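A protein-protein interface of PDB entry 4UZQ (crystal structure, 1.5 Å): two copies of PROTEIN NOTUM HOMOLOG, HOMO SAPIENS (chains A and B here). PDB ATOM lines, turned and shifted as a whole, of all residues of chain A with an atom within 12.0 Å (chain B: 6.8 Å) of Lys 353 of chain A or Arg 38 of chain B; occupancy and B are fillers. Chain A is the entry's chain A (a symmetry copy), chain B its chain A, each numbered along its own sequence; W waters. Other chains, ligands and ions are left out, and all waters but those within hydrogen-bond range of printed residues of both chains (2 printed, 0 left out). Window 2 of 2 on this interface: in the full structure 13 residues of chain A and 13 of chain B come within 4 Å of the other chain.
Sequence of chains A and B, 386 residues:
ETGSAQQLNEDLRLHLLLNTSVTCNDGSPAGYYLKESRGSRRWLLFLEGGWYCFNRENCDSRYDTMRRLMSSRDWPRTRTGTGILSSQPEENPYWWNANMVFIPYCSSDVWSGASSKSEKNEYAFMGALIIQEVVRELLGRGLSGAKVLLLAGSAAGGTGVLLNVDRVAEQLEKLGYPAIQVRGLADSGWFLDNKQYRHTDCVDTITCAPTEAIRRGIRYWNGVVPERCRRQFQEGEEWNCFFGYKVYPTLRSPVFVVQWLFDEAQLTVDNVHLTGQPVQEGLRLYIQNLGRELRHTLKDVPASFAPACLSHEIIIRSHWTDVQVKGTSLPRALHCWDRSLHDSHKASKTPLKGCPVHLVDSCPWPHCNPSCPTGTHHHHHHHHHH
No position is printed for both chains.
Of the 13 printed residues of chain B, 4 touch a printed residue of chain A.
Printed residues of chain B that touch a printed residue of chain A: Arg 38, Gly 39, Arg 41 and Asn 97.
Among the printed residues, no Asp or Glu carboxylate lies within 4 Å of a Lys or Arg side-chain nitrogen of the other chain.
The side-chain carboxylate (OE1) of Glu 36 of chain B is in salt-bridge range of the guanidinium group (NE) of Arg 38 of chain B, 3.2 Å away.
The side-chain hydroxyl (OG) of Ser 37 of chain B lies within hydrogen-bond range of the backbone carbonyl oxygen (O) of Asn 97 of chain B (2.6 Å).
The guanidinium group (NH2) of Arg 38 of chain B is in hydrogen-bond range of the backbone carbonyl oxygen (O) of Arg 141 of chain B (3.4 Å).
NH1 of Arg 332 of chain A lies within hydrogen-bond range of SG of Cys 355 of chain A (3.7 Å).
SG of Cys 355 of chain A forms a disulfide with SG of Cys 336 of chain A (2.0 Å).
The guanidinium group of Arg 339 of chain A lies within hydrogen-bond range of the side-chain sulfur of Cys 355 of chain A (3.6 Å).
O of Gly 39 of chain B is in hydrogen-bond range of NE2 of His 335 of chain A.
The backbone carbonyl oxygen (O) of Gly 39 of chain B is in hydrogen-bond range of the guanidinium group (NH1) of Arg 339 of chain A, at 3.1 Å.
Water W1 bridges O of Arg 38 of chain B (2.6 Å) and O of Lys 353 of chain A (3.2 Å).
Water W2 bridges the side-chain amide oxygen of Asn 97 of chain B (2.8 Å) and the side-chain hydroxyl of Tyr 94 of chain A (3.2 Å).
Among the printed residues, pairs that only touch across the chains: Lys 353 of chain A with Arg 38 of chain B (3.6 Å), Tyr 94 of chain A with Asn 97 of chain B (3.8 Å), Arg 339 of chain A with Arg 38 of chain B (3.9 Å), Arg 339 of chain A with Arg 41 of chain B (3.9 Å) and Cys 355 of chain A with Gly 39 of chain B (3.9 Å).
Of the printed residues of chain B, Arg 339 of chain A touches Arg 38 (3.9 Å), Gly 39 (3.1 Å) and Arg 41 (3.9 Å).
Printed residues of chain B within 4 Å of Lys 353 of chain A: Arg 38 (3.6 Å).
Printed residues of chain B within 4 Å of Cys 355 of chain A: Gly 39.
Pro 356 of chain A touches none of the printed residues of chain B.
Val 357 of chain A touches none of the printed residues of chain B.
No residue of chain A comes within 4 Å of Glu 36 of chain B.
Ser 37 of chain B touches none of the printed residues of chain A.
Of the printed residues of chain A, Arg 38 of chain B touches Arg 339 (3.9 Å) and Lys 353 (3.6 Å).
Printed residues of chain A within 4 Å of Gly 39 of chain B: His 335, Arg 339 and Cys 355.
No residue of chain A comes within 4 Å of Ser 40 of chain B.
Of the printed residues of chain A, Arg 41 of chain B touches Arg 339.
Of the printed residues of chain A, Asn 97 of chain B touches Tyr 94.
No residue of chain A comes within 4 Å of Gly 142 of chain B.
The nearest residue of chain B that does not touch Lys 353 of chain A is Gly 39 of chain B (5.1 Å).
The nearest printed residue of chain A that does not touch Arg 38 of chain B is Gly 354 of chain A (4.7 Å).
The nearest printed residue of chain B that does not touch His 335 of chain A is Asn 97 of chain B (4.1 Å).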
ATOM      1  N   TYR A  94      21.422  14.670  36.997  1.00  0.00           N
ATOM      2  CA  TYR A  94      21.226  14.420  35.584  1.00  0.00           C
ATOM      3  C   TYR A  94      21.496  12.977  35.238  1.00  0.00           C
ATOM      4  O   TYR A  94      20.722  12.397  34.463  1.00  0.00           O
ATOM      5  CB  TYR A  94      22.066  15.278  34.702  1.00  0.00           C
ATOM      6  CG  TYR A  94      21.849  16.738  34.842  1.00  0.00           C
ATOM      7  CD1 TYR A  94      22.518  17.452  35.821  1.00  0.00           C
ATOM      8  CD2 TYR A  94      20.853  17.424  34.136  1.00  0.00           C
ATOM      9  CE1 TYR A  94      22.342  18.824  35.981  1.00  0.00           C
ATOM     10  CE2 TYR A  94      20.701  18.778  34.280  1.00  0.00           C
ATOM     11  CZ  TYR A  94      21.421  19.493  35.209  1.00  0.00           C
ATOM     12  OH  TYR A  94      21.233  20.862  35.407  1.00  0.00           O
ATOM     13  N   GLY A 327      28.393  31.132  38.377  1.00  0.00           N
ATOM     14  CA  GLY A 327      26.972  30.801  38.610  1.00  0.00           C
ATOM     15  C   GLY A 327      26.421  29.419  38.249  1.00  0.00           C
ATOM     16  O   GLY A 327      25.216  29.138  38.443  1.00  0.00           O
ATOM     17  N   THR A 328      27.288  28.553  37.749  1.00  0.00           N
ATOM     18  CA  THR A 328      26.914  27.230  37.262  1.00  0.00           C
ATOM     19  C   THR A 328      27.656  26.121  37.995  1.00  0.00           C
ATOM     20  O   THR A 328      28.856  26.211  38.204  1.00  0.00           O
ATOM     21  CB  THR A 328      27.117  27.152  35.730  1.00  0.00           C
ATOM     22  OG1 THR A 328      26.322  28.136  35.115  1.00  0.00           O
ATOM     23  CG2 THR A 328      26.827  25.799  35.105  1.00  0.00           C
ATOM     24  N   ARG A 332      25.567  20.535  36.052  1.00  0.00           N
ATOM     25  CA  ARG A 332      24.882  21.269  34.979  1.00  0.00           C
ATOM     26  C   ARG A 332      25.781  21.499  33.775  1.00  0.00           C
ATOM     27  O   ARG A 332      25.368  21.337  32.624  1.00  0.00           O
ATOM     28  CB  ARG A 332      24.322  22.598  35.476  1.00  0.00           C
ATOM     29  CG  ARG A 332      23.540  23.356  34.403  1.00  0.00           C
ATOM     30  CD  ARG A 332      22.622  24.364  35.034  1.00  0.00           C
ATOM     31  NE  ARG A 332      22.868  25.718  34.583  1.00  0.00           N
ATOM     32  CZ  ARG A 332      22.501  26.212  33.400  1.00  0.00           C
ATOM     33  NH1 ARG A 332      21.895  25.454  32.473  1.00  0.00           N
ATOM     34  NH2 ARG A 332      22.756  27.488  33.130  1.00  0.00           N
ATOM     35  N   ALA A 333      27.016  21.950  34.037  1.00  0.00           N
ATOM     36  CA  ALA A 333      27.992  22.147  32.933  1.00  0.00           C
ATOM     37  C   ALA A 333      28.146  20.846  32.136  1.00  0.00           C
ATOM     38  O   ALA A 333      28.216  20.860  30.902  1.00  0.00           O
ATOM     39  CB  ALA A 333      29.380  22.590  33.442  1.00  0.00           C
ATOM     40  N   HIS A 335      25.914  18.366  31.818  1.00  0.00           N
ATOM     41  CA  HIS A 335      24.729  18.230  31.070  1.00  0.00           C
ATOM     42  C   HIS A 335      24.749  19.134  29.847  1.00  0.00           C
ATOM     43  O   HIS A 335      24.360  18.701  28.736  1.00  0.00           O
ATOM     44  CB  HIS A 335      23.515  18.589  31.971  1.00  0.00           C
ATOM     45  CG  HIS A 335      22.254  18.909  31.214  1.00  0.00           C
ATOM     46  ND1 HIS A 335      21.484  17.951  30.587  1.00  0.00           N
ATOM     47  CD2 HIS A 335      21.675  20.103  30.943  1.00  0.00           C
ATOM     48  CE1 HIS A 335      20.470  18.537  29.967  1.00  0.00           C
ATOM     49  NE2 HIS A 335      20.556  19.842  30.167  1.00  0.00           N
ATOM     50  N   CYS A 336      25.134  20.401  30.009  1.00  0.00           N
ATOM     51  CA  CYS A 336      25.220  21.316  28.865  1.00  0.00           C
ATOM     52  C   CYS A 336      26.188  20.808  27.781  1.00  0.00           C
ATOM     53  O   CYS A 336      25.890  20.893  26.557  1.00  0.00           O
ATOM     54  CB  CYS A 336      25.595  22.708  29.292  1.00  0.00           C
ATOM     55  SG  CYS A 336      24.392  23.488  30.387  1.00  0.00           S
ATOM     56  N   TRP A 337      27.302  20.245  28.212  1.00  0.00           N
ATOM     57  CA  TRP A 337      28.242  19.668  27.272  1.00  0.00           C
ATOM     58  C   TRP A 337      27.654  18.499  26.533  1.00  0.00           C
ATOM     59  O   TRP A 337      27.774  18.457  25.310  1.00  0.00           O
ATOM     60  CB  TRP A 337      29.491  19.252  28.050  1.00  0.00           C
ATOM     61  CG  TRP A 337      30.536  18.521  27.327  1.00  0.00           C
ATOM     62  CD1 TRP A 337      31.317  18.962  26.332  1.00  0.00           C
ATOM     63  CD2 TRP A 337      31.001  17.236  27.697  1.00  0.00           C
ATOM     64  NE1 TRP A 337      32.228  17.968  26.002  1.00  0.00           N
ATOM     65  CE2 TRP A 337      32.068  16.909  26.851  1.00  0.00           C
ATOM     66  CE3 TRP A 337      30.651  16.338  28.711  1.00  0.00           C
ATOM     67  CZ2 TRP A 337      32.733  15.685  26.934  1.00  0.00           C
ATOM     68  CZ3 TRP A 337      31.379  15.099  28.822  1.00  0.00           C
ATOM     69  CH2 TRP A 337      32.395  14.818  27.932  1.00  0.00           C
ATOM     70  N   ASP A 338      27.065  17.557  27.253  1.00  0.00           N
ATOM     71  CA  ASP A 338      26.357  16.411  26.628  1.00  0.00           C
ATOM     72  C   ASP A 338      25.359  16.899  25.548  1.00  0.00           C
ATOM     73  O   ASP A 338      25.348  16.392  24.418  1.00  0.00           O
ATOM     74  CB  ASP A 338      25.669  15.588  27.728  1.00  0.00           C
ATOM     75  CG  ASP A 338      24.876  14.445  27.201  1.00  0.00           C
ATOM     76  OD1 ASP A 338      25.396  13.388  26.951  1.00  0.00           O
ATOM     77  OD2 ASP A 338      23.661  14.607  27.162  1.00  0.00           O
ATOM     78  N   ARG A 339      24.569  17.922  25.860  1.00  0.00           N
ATOM     79  CA  ARG A 339      23.591  18.479  24.903  1.00  0.00           C
ATOM     80  C   ARG A 339      24.269  19.094  23.707  1.00  0.00           C
ATOM     81  O   ARG A 339      23.819  18.915  22.558  1.00  0.00           O
ATOM     82  CB  ARG A 339      22.754  19.569  25.561  1.00  0.00           C
ATOM     83  CG  ARG A 339      21.476  19.084  26.228  1.00  0.00           C
ATOM     84  CD  ARG A 339      20.627  20.265  26.627  1.00  0.00           C
ATOM     85  NE  ARG A 339      20.121  21.062  25.517  1.00  0.00           N
ATOM     86  CZ  ARG A 339      19.928  22.358  25.622  1.00  0.00           C
ATOM     87  NH1 ARG A 339      20.258  22.928  26.736  1.00  0.00           N
ATOM     88  NH2 ARG A 339      19.438  23.067  24.634  1.00  0.00           N
ATOM     89  N   SER A 340      25.419  19.770  23.961  1.00  0.00           N
ATOM     90  CA  SER A 340      26.149  20.433  22.874  1.00  0.00           C
ATOM     91  C   SER A 340      26.671  19.401  21.922  1.00  0.00           C
ATOM     92  O   SER A 340      26.767  19.703  20.757  1.00  0.00           O
ATOM     93  CB  SER A 340      27.297  21.316  23.362  1.00  0.00           C
ATOM     94  OG  SER A 340      28.364  20.514  23.871  1.00  0.00           O
ATOM     95  N   LEU A 341      26.968  18.202  22.378  1.00  0.00           N
ATOM     96  CA  LEU A 341      27.584  17.179  21.515  1.00  0.00           C
ATOM     97  C   LEU A 341      26.509  16.442  20.724  1.00  0.00           C
ATOM     98  O   LEU A 341      26.764  15.862  19.688  1.00  0.00           O
ATOM     99  CB  LEU A 341      28.359  16.174  22.336  1.00  0.00           C
ATOM    100  CG  LEU A 341      29.647  16.746  22.947  1.00  0.00           C
ATOM    101  CD1 LEU A 341      30.233  15.736  23.908  1.00  0.00           C
ATOM    102  CD2 LEU A 341      30.695  17.142  21.919  1.00  0.00           C
ATOM    103  N   HIS A 342      25.318  16.405  21.281  1.00  0.00           N
ATOM    104  CA  HIS A 342      24.166  15.885  20.586  1.00  0.00           C
ATOM    105  C   HIS A 342      23.751  16.892  19.513  1.00  0.00           C
ATOM    106  O   HIS A 342      24.177  16.785  18.376  1.00  0.00           O
ATOM    107  CB  HIS A 342      23.031  15.702  21.611  1.00  0.00           C
ATOM    108  CG  HIS A 342      21.834  15.001  21.090  1.00  0.00           C
ATOM    109  ND1 HIS A 342      20.741  15.672  20.583  1.00  0.00           N
ATOM    110  CD2 HIS A 342      21.521  13.686  21.045  1.00  0.00           C
ATOM    111  CE1 HIS A 342      19.823  14.798  20.210  1.00  0.00           C
ATOM    112  NE2 HIS A 342      20.267  13.586  20.489  1.00  0.00           N
ATOM    113  N   LYS A 353      22.208  27.771  24.203  1.00  0.00           N
ATOM    114  CA  LYS A 353      21.489  28.954  24.811  1.00  0.00           C
ATOM    115  C   LYS A 353      21.186  28.767  26.311  1.00  0.00           C
ATOM    116  O   LYS A 353      20.469  27.883  26.678  1.00  0.00           O
ATOM    117  CB  LYS A 353      20.184  29.252  24.034  1.00  0.00           C
ATOM    118  CG  LYS A 353      19.165  30.127  24.786  1.00  0.00           C
ATOM    119  CD  LYS A 353      17.845  30.340  24.034  1.00  0.00           C
ATOM    120  CE  LYS A 353      17.960  31.495  23.050  1.00  0.00           C
ATOM    121  NZ  LYS A 353      16.647  31.963  22.485  1.00  0.00           N
ATOM    122  N   GLY A 354      21.817  29.569  27.166  1.00  0.00           N
ATOM    123  CA  GLY A 354      21.628  29.478  28.635  1.00  0.00           C
ATOM    124  C   GLY A 354      22.235  28.200  29.245  1.00  0.00           C
ATOM    125  O   GLY A 354      21.809  27.724  30.298  1.00  0.00           O
ATOM    126  N   CYS A 355      23.236  27.643  28.585  1.00  0.00           N
ATOM    127  CA  CYS A 355      23.772  26.359  29.063  1.00  0.00           C
ATOM    128  C   CYS A 355      25.295  26.343  28.821  1.00  0.00           C
ATOM    129  O   CYS A 355      25.789  25.823  27.803  1.00  0.00           O
ATOM    130  CB  CYS A 355      23.059  25.213  28.352  1.00  0.00           C
ATOM    131  SG  CYS A 355      22.723  23.693  29.286  1.00  0.00           S
ATOM    132  N   PRO A 356      26.059  26.921  29.758  1.00  0.00           N
ATOM    133  CA  PRO A 356      27.483  27.076  29.574  1.00  0.00           C
ATOM    134  C   PRO A 356      28.260  25.788  29.782  1.00  0.00           C
ATOM    135  O   PRO A 356      27.874  24.910  30.600  1.00  0.00           O
ATOM    136  CB  PRO A 356      27.859  28.068  30.613  1.00  0.00           C
ATOM    137  CG  PRO A 356      26.868  27.939  31.673  1.00  0.00           C
ATOM    138  CD  PRO A 356      25.599  27.485  31.023  1.00  0.00           C
ATOM    139  N   VAL A 357      29.377  25.701  29.032  1.00  0.00           N
ATOM    140  CA  VAL A 357      30.292  24.555  29.139  1.00  0.00           C
ATOM    141  C   VAL A 357      31.734  24.942  29.478  1.00  0.00           C
ATOM    142  O   VAL A 357      32.506  24.075  29.897  1.00  0.00           O
ATOM    143  CB  VAL A 357      30.317  23.677  27.877  1.00  0.00           C
ATOM    144  CG1 VAL A 357      28.939  23.133  27.635  1.00  0.00           C
ATOM    145  CG2 VAL A 357      30.812  24.431  26.661  1.00  0.00           C
ATOM    146  N   HIS A 358      32.079  26.214  29.227  1.00  0.00           N
ATOM    147  CA  HIS A 358      33.411  26.728  29.511  1.00  0.00           C
ATOM    148  C   HIS A 358      33.386  27.689  30.698  1.00  0.00           C
ATOM    149  O   HIS A 358      32.954  28.844  30.567  1.00  0.00           O
ATOM    150  CB  HIS A 358      33.966  27.445  28.270  1.00  0.00           C
ATOM    151  CG  HIS A 358      35.407  27.792  28.396  1.00  0.00           C
ATOM    152  ND1 HIS A 358      36.399  26.865  28.144  1.00  0.00           N
ATOM    153  CD2 HIS A 358      36.033  28.937  28.768  1.00  0.00           C
ATOM    154  CE1 HIS A 358      37.582  27.439  28.333  1.00  0.00           C
ATOM    155  NE2 HIS A 358      37.384  28.699  28.706  1.00  0.00           N
ATOM    156  N   LEU A 359      33.883  27.189  31.854  1.00  0.00           N
ATOM    157  CA  LEU A 359      33.680  27.804  33.123  1.00  0.00           C
ATOM    158  C   LEU A 359      35.020  27.807  33.922  1.00  0.00           C
ATOM    159  O   LEU A 359      35.364  26.881  34.653  1.00  0.00           O
ATOM    160  CB  LEU A 359      32.604  27.060  33.926  1.00  0.00           C
ATOM    161  CG  LEU A 359      31.224  27.157  33.267  1.00  0.00           C
ATOM    162  CD1 LEU A 359      30.351  26.084  33.827  1.00  0.00           C
ATOM    163  CD2 LEU A 359      30.637  28.561  33.492  1.00  0.00           C
ATOM    164  N   GLU B  36      10.468  28.471  33.705  1.00  0.00           N
ATOM    165  CA  GLU B  36      11.410  28.177  32.611  1.00  0.00           C
ATOM    166  C   GLU B  36      12.626  27.348  33.065  1.00  0.00           C
ATOM    167  O   GLU B  36      13.073  27.483  34.177  1.00  0.00           O
ATOM    168  CB  GLU B  36      11.949  29.509  32.041  1.00  0.00           C
ATOM    169  CG  GLU B  36      10.925  30.289  31.266  1.00  0.00           C
ATOM    170  CD  GLU B  36      11.015  30.131  29.768  1.00  0.00           C
ATOM    171  OE1 GLU B  36      11.839  29.302  29.273  1.00  0.00           O
ATOM    172  OE2 GLU B  36      10.220  30.835  29.111  1.00  0.00           O
ATOM    173  N   SER B  37      13.083  26.455  32.186  1.00  0.00           N
ATOM    174  CA  SER B  37      14.271  25.709  32.351  1.00  0.00           C
ATOM    175  C   SER B  37      15.057  25.724  31.036  1.00  0.00           C
ATOM    176  O   SER B  37      14.901  24.877  30.103  1.00  0.00           O
ATOM    177  CB  SER B  37      13.991  24.295  32.759  1.00  0.00           C
ATOM    178  OG  SER B  37      15.216  23.664  33.068  1.00  0.00           O
ATOM    179  N   ARG B  38      15.913  26.711  30.958  1.00  0.00           N
ATOM    180  CA  ARG B  38      16.607  26.919  29.687  1.00  0.00           C
ATOM    181  C   ARG B  38      17.556  25.838  29.229  1.00  0.00           C
ATOM    182  O   ARG B  38      17.850  25.747  28.009  1.00  0.00           O
ATOM    183  CB  ARG B  38      17.202  28.289  29.646  1.00  0.00           C
ATOM    184  CG  ARG B  38      16.095  29.337  29.575  1.00  0.00           C
ATOM    185  CD  ARG B  38      15.543  29.597  28.174  1.00  0.00           C
ATOM    186  NE  ARG B  38      14.513  30.635  28.230  1.00  0.00           N
ATOM    187  CZ  ARG B  38      13.900  31.182  27.169  1.00  0.00           C
ATOM    188  NH1 ARG B  38      14.206  30.838  25.907  1.00  0.00           N
ATOM    189  NH2 ARG B  38      12.985  32.122  27.375  1.00  0.00           N
ATOM    190  N   GLY B  39      18.011  24.984  30.146  1.00  0.00           N
ATOM    191  CA  GLY B  39      18.806  23.845  29.731  1.00  0.00           C
ATOM    192  C   GLY B  39      18.061  22.615  29.270  1.00  0.00           C
ATOM    193  O   GLY B  39      18.666  21.576  29.060  1.00  0.00           O
ATOM    194  N   SER B  40      16.711  22.703  29.210  1.00  0.00           N
ATOM    195  CA  SER B  40      15.921  21.566  28.746  1.00  0.00           C
ATOM    196  C   SER B  40      15.063  21.926  27.588  1.00  0.00           C
ATOM    197  O   SER B  40      14.588  23.052  27.504  1.00  0.00           O
ATOM    198  CB  SER B  40      14.976  21.127  29.880  1.00  0.00           C
ATOM    199  OG  SER B  40      14.053  20.089  29.520  1.00  0.00           O
ATOM    200  N   ARG B  41      14.916  20.962  26.690  1.00  0.00           N
ATOM    201  CA  ARG B  41      13.994  21.093  25.559  1.00  0.00           C
ATOM    202  C   ARG B  41      12.662  20.365  25.846  1.00  0.00           C
ATOM    203  O   ARG B  41      11.871  20.151  24.913  1.00  0.00           O
ATOM    204  CB  ARG B  41      14.656  20.673  24.245  1.00  0.00           C
ATOM    205  CG  ARG B  41      15.881  21.533  23.921  1.00  0.00           C
ATOM    206  CD  ARG B  41      16.536  21.086  22.660  1.00  0.00           C
ATOM    207  NE  ARG B  41      15.635  21.332  21.556  1.00  0.00           N
ATOM    208  CZ  ARG B  41      15.785  20.831  20.341  1.00  0.00           C
ATOM    209  NH1 ARG B  41      16.817  20.059  20.073  1.00  0.00           N
ATOM    210  NH2 ARG B  41      14.890  21.098  19.404  1.00  0.00           N
ATOM    211  N   TRP B  43       9.027  20.229  27.631  1.00  0.00           N
ATOM    212  CA  TRP B  43       7.963  21.036  28.240  1.00  0.00           C
ATOM    213  C   TRP B  43       6.818  20.138  28.747  1.00  0.00           C
ATOM    214  O   TRP B  43       6.341  19.254  28.007  1.00  0.00           O
ATOM    215  CB  TRP B  43       7.397  22.019  27.188  1.00  0.00           C
ATOM    216  CG  TRP B  43       8.365  23.117  26.866  1.00  0.00           C
ATOM    217  CD1 TRP B  43       9.557  23.020  26.225  1.00  0.00           C
ATOM    218  CD2 TRP B  43       8.218  24.464  27.232  1.00  0.00           C
ATOM    219  NE1 TRP B  43      10.149  24.234  26.207  1.00  0.00           N
ATOM    220  CE2 TRP B  43       9.349  25.149  26.808  1.00  0.00           C
ATOM    221  CE3 TRP B  43       7.238  25.157  27.933  1.00  0.00           C
ATOM    222  CZ2 TRP B  43       9.560  26.488  27.085  1.00  0.00           C
ATOM    223  CZ3 TRP B  43       7.408  26.472  28.153  1.00  0.00           C
ATOM    224  CH2 TRP B  43       8.560  27.172  27.713  1.00  0.00           C
ATOM    225  N   ASN B  97      14.086  18.656  35.472  1.00  0.00           N
ATOM    226  CA  ASN B  97      14.629  19.807  34.774  1.00  0.00           C
ATOM    227  C   ASN B  97      13.788  20.370  33.642  1.00  0.00           C
ATOM    228  O   ASN B  97      14.200  21.267  32.905  1.00  0.00           O
ATOM    229  CB  ASN B  97      16.020  19.454  34.241  1.00  0.00           C
ATOM    230  CG  ASN B  97      16.857  20.658  33.928  1.00  0.00           C
ATOM    231  OD1 ASN B  97      16.841  21.650  34.627  1.00  0.00           O
ATOM    232  ND2 ASN B  97      17.640  20.543  32.918  1.00  0.00           N
ATOM    233  N   ASN B  99      10.791  22.381  31.494  1.00  0.00           N
ATOM    234  CA  ASN B  99      10.009  23.626  31.523  1.00  0.00           C
ATOM    235  C   ASN B  99       8.607  23.255  32.011  1.00  0.00           C
ATOM    236  O   ASN B  99       8.023  22.375  31.431  1.00  0.00           O
ATOM    237  CB  ASN B  99       9.934  24.224  30.143  1.00  0.00           C
ATOM    238  CG  ASN B  99      11.298  24.691  29.640  1.00  0.00           C
ATOM    239  OD1 ASN B  99      11.750  25.817  29.913  1.00  0.00           O
ATOM    240  ND2 ASN B  99      11.969  23.763  29.004  1.00  0.00           N
ATOM    241  N   GLY B 140       6.562  32.243  22.238  1.00  0.00           N
ATOM    242  CA  GLY B 140       7.441  33.398  22.423  1.00  0.00           C
ATOM    243  C   GLY B 140       8.235  33.356  23.701  1.00  0.00           C
ATOM    244  O   GLY B 140       8.899  34.315  24.014  1.00  0.00           O
ATOM    245  N   ARG B 141       8.166  32.237  24.426  1.00  0.00           N
ATOM    246  CA  ARG B 141       8.847  32.073  25.704  1.00  0.00           C
ATOM    247  C   ARG B 141       9.723  30.815  25.745  1.00  0.00           C
ATOM    248  O   ARG B 141      10.157  30.370  26.816  1.00  0.00           O
ATOM    249  CB  ARG B 141       7.862  32.063  26.879  1.00  0.00           C
ATOM    250  CG  ARG B 141       7.147  33.404  27.056  1.00  0.00           C
ATOM    251  CD  ARG B 141       6.202  33.360  28.268  1.00  0.00           C
ATOM    252  NE  ARG B 141       5.598  34.630  28.689  1.00  0.00           N
ATOM    253  CZ  ARG B 141       6.151  35.540  29.494  1.00  0.00           C
ATOM    254  NH1 ARG B 141       7.403  35.419  30.009  1.00  0.00           N
ATOM    255  NH2 ARG B 141       5.415  36.620  29.787  1.00  0.00           N
ATOM    256  N   GLY B 142      10.017  30.246  24.591  1.00  0.00           N
ATOM    257  CA  GLY B 142      10.907  29.135  24.609  1.00  0.00           C
ATOM    258  C   GLY B 142      10.376  27.895  23.998  1.00  0.00           C
ATOM    259  O   GLY B 142      11.152  27.017  23.629  1.00  0.00           O
ATOM    260  N   LEU B 143       9.045  27.769  23.945  1.00  0.00           N
ATOM    261  CA  LEU B 143       8.485  26.529  23.436  1.00  0.00           C
ATOM    262  C   LEU B 143       8.824  26.279  21.962  1.00  0.00           C
ATOM    263  O   LEU B 143       8.882  25.128  21.529  1.00  0.00           O
ATOM    264  CB  LEU B 143       6.956  26.549  23.656  1.00  0.00           C
ATOM    265  CG  LEU B 143       6.166  25.333  23.159  1.00  0.00           C
ATOM    266  CD1 LEU B 143       6.562  24.107  23.954  1.00  0.00           C
ATOM    267  CD2 LEU B 143       4.669  25.561  23.257  1.00  0.00           C
HETATM  268  O   HOH W   1      17.418  27.341  25.950  1.00  0.00           O
HETATM  269  O   HOH W   2      18.915  23.015  35.865  1.00  0.00           O
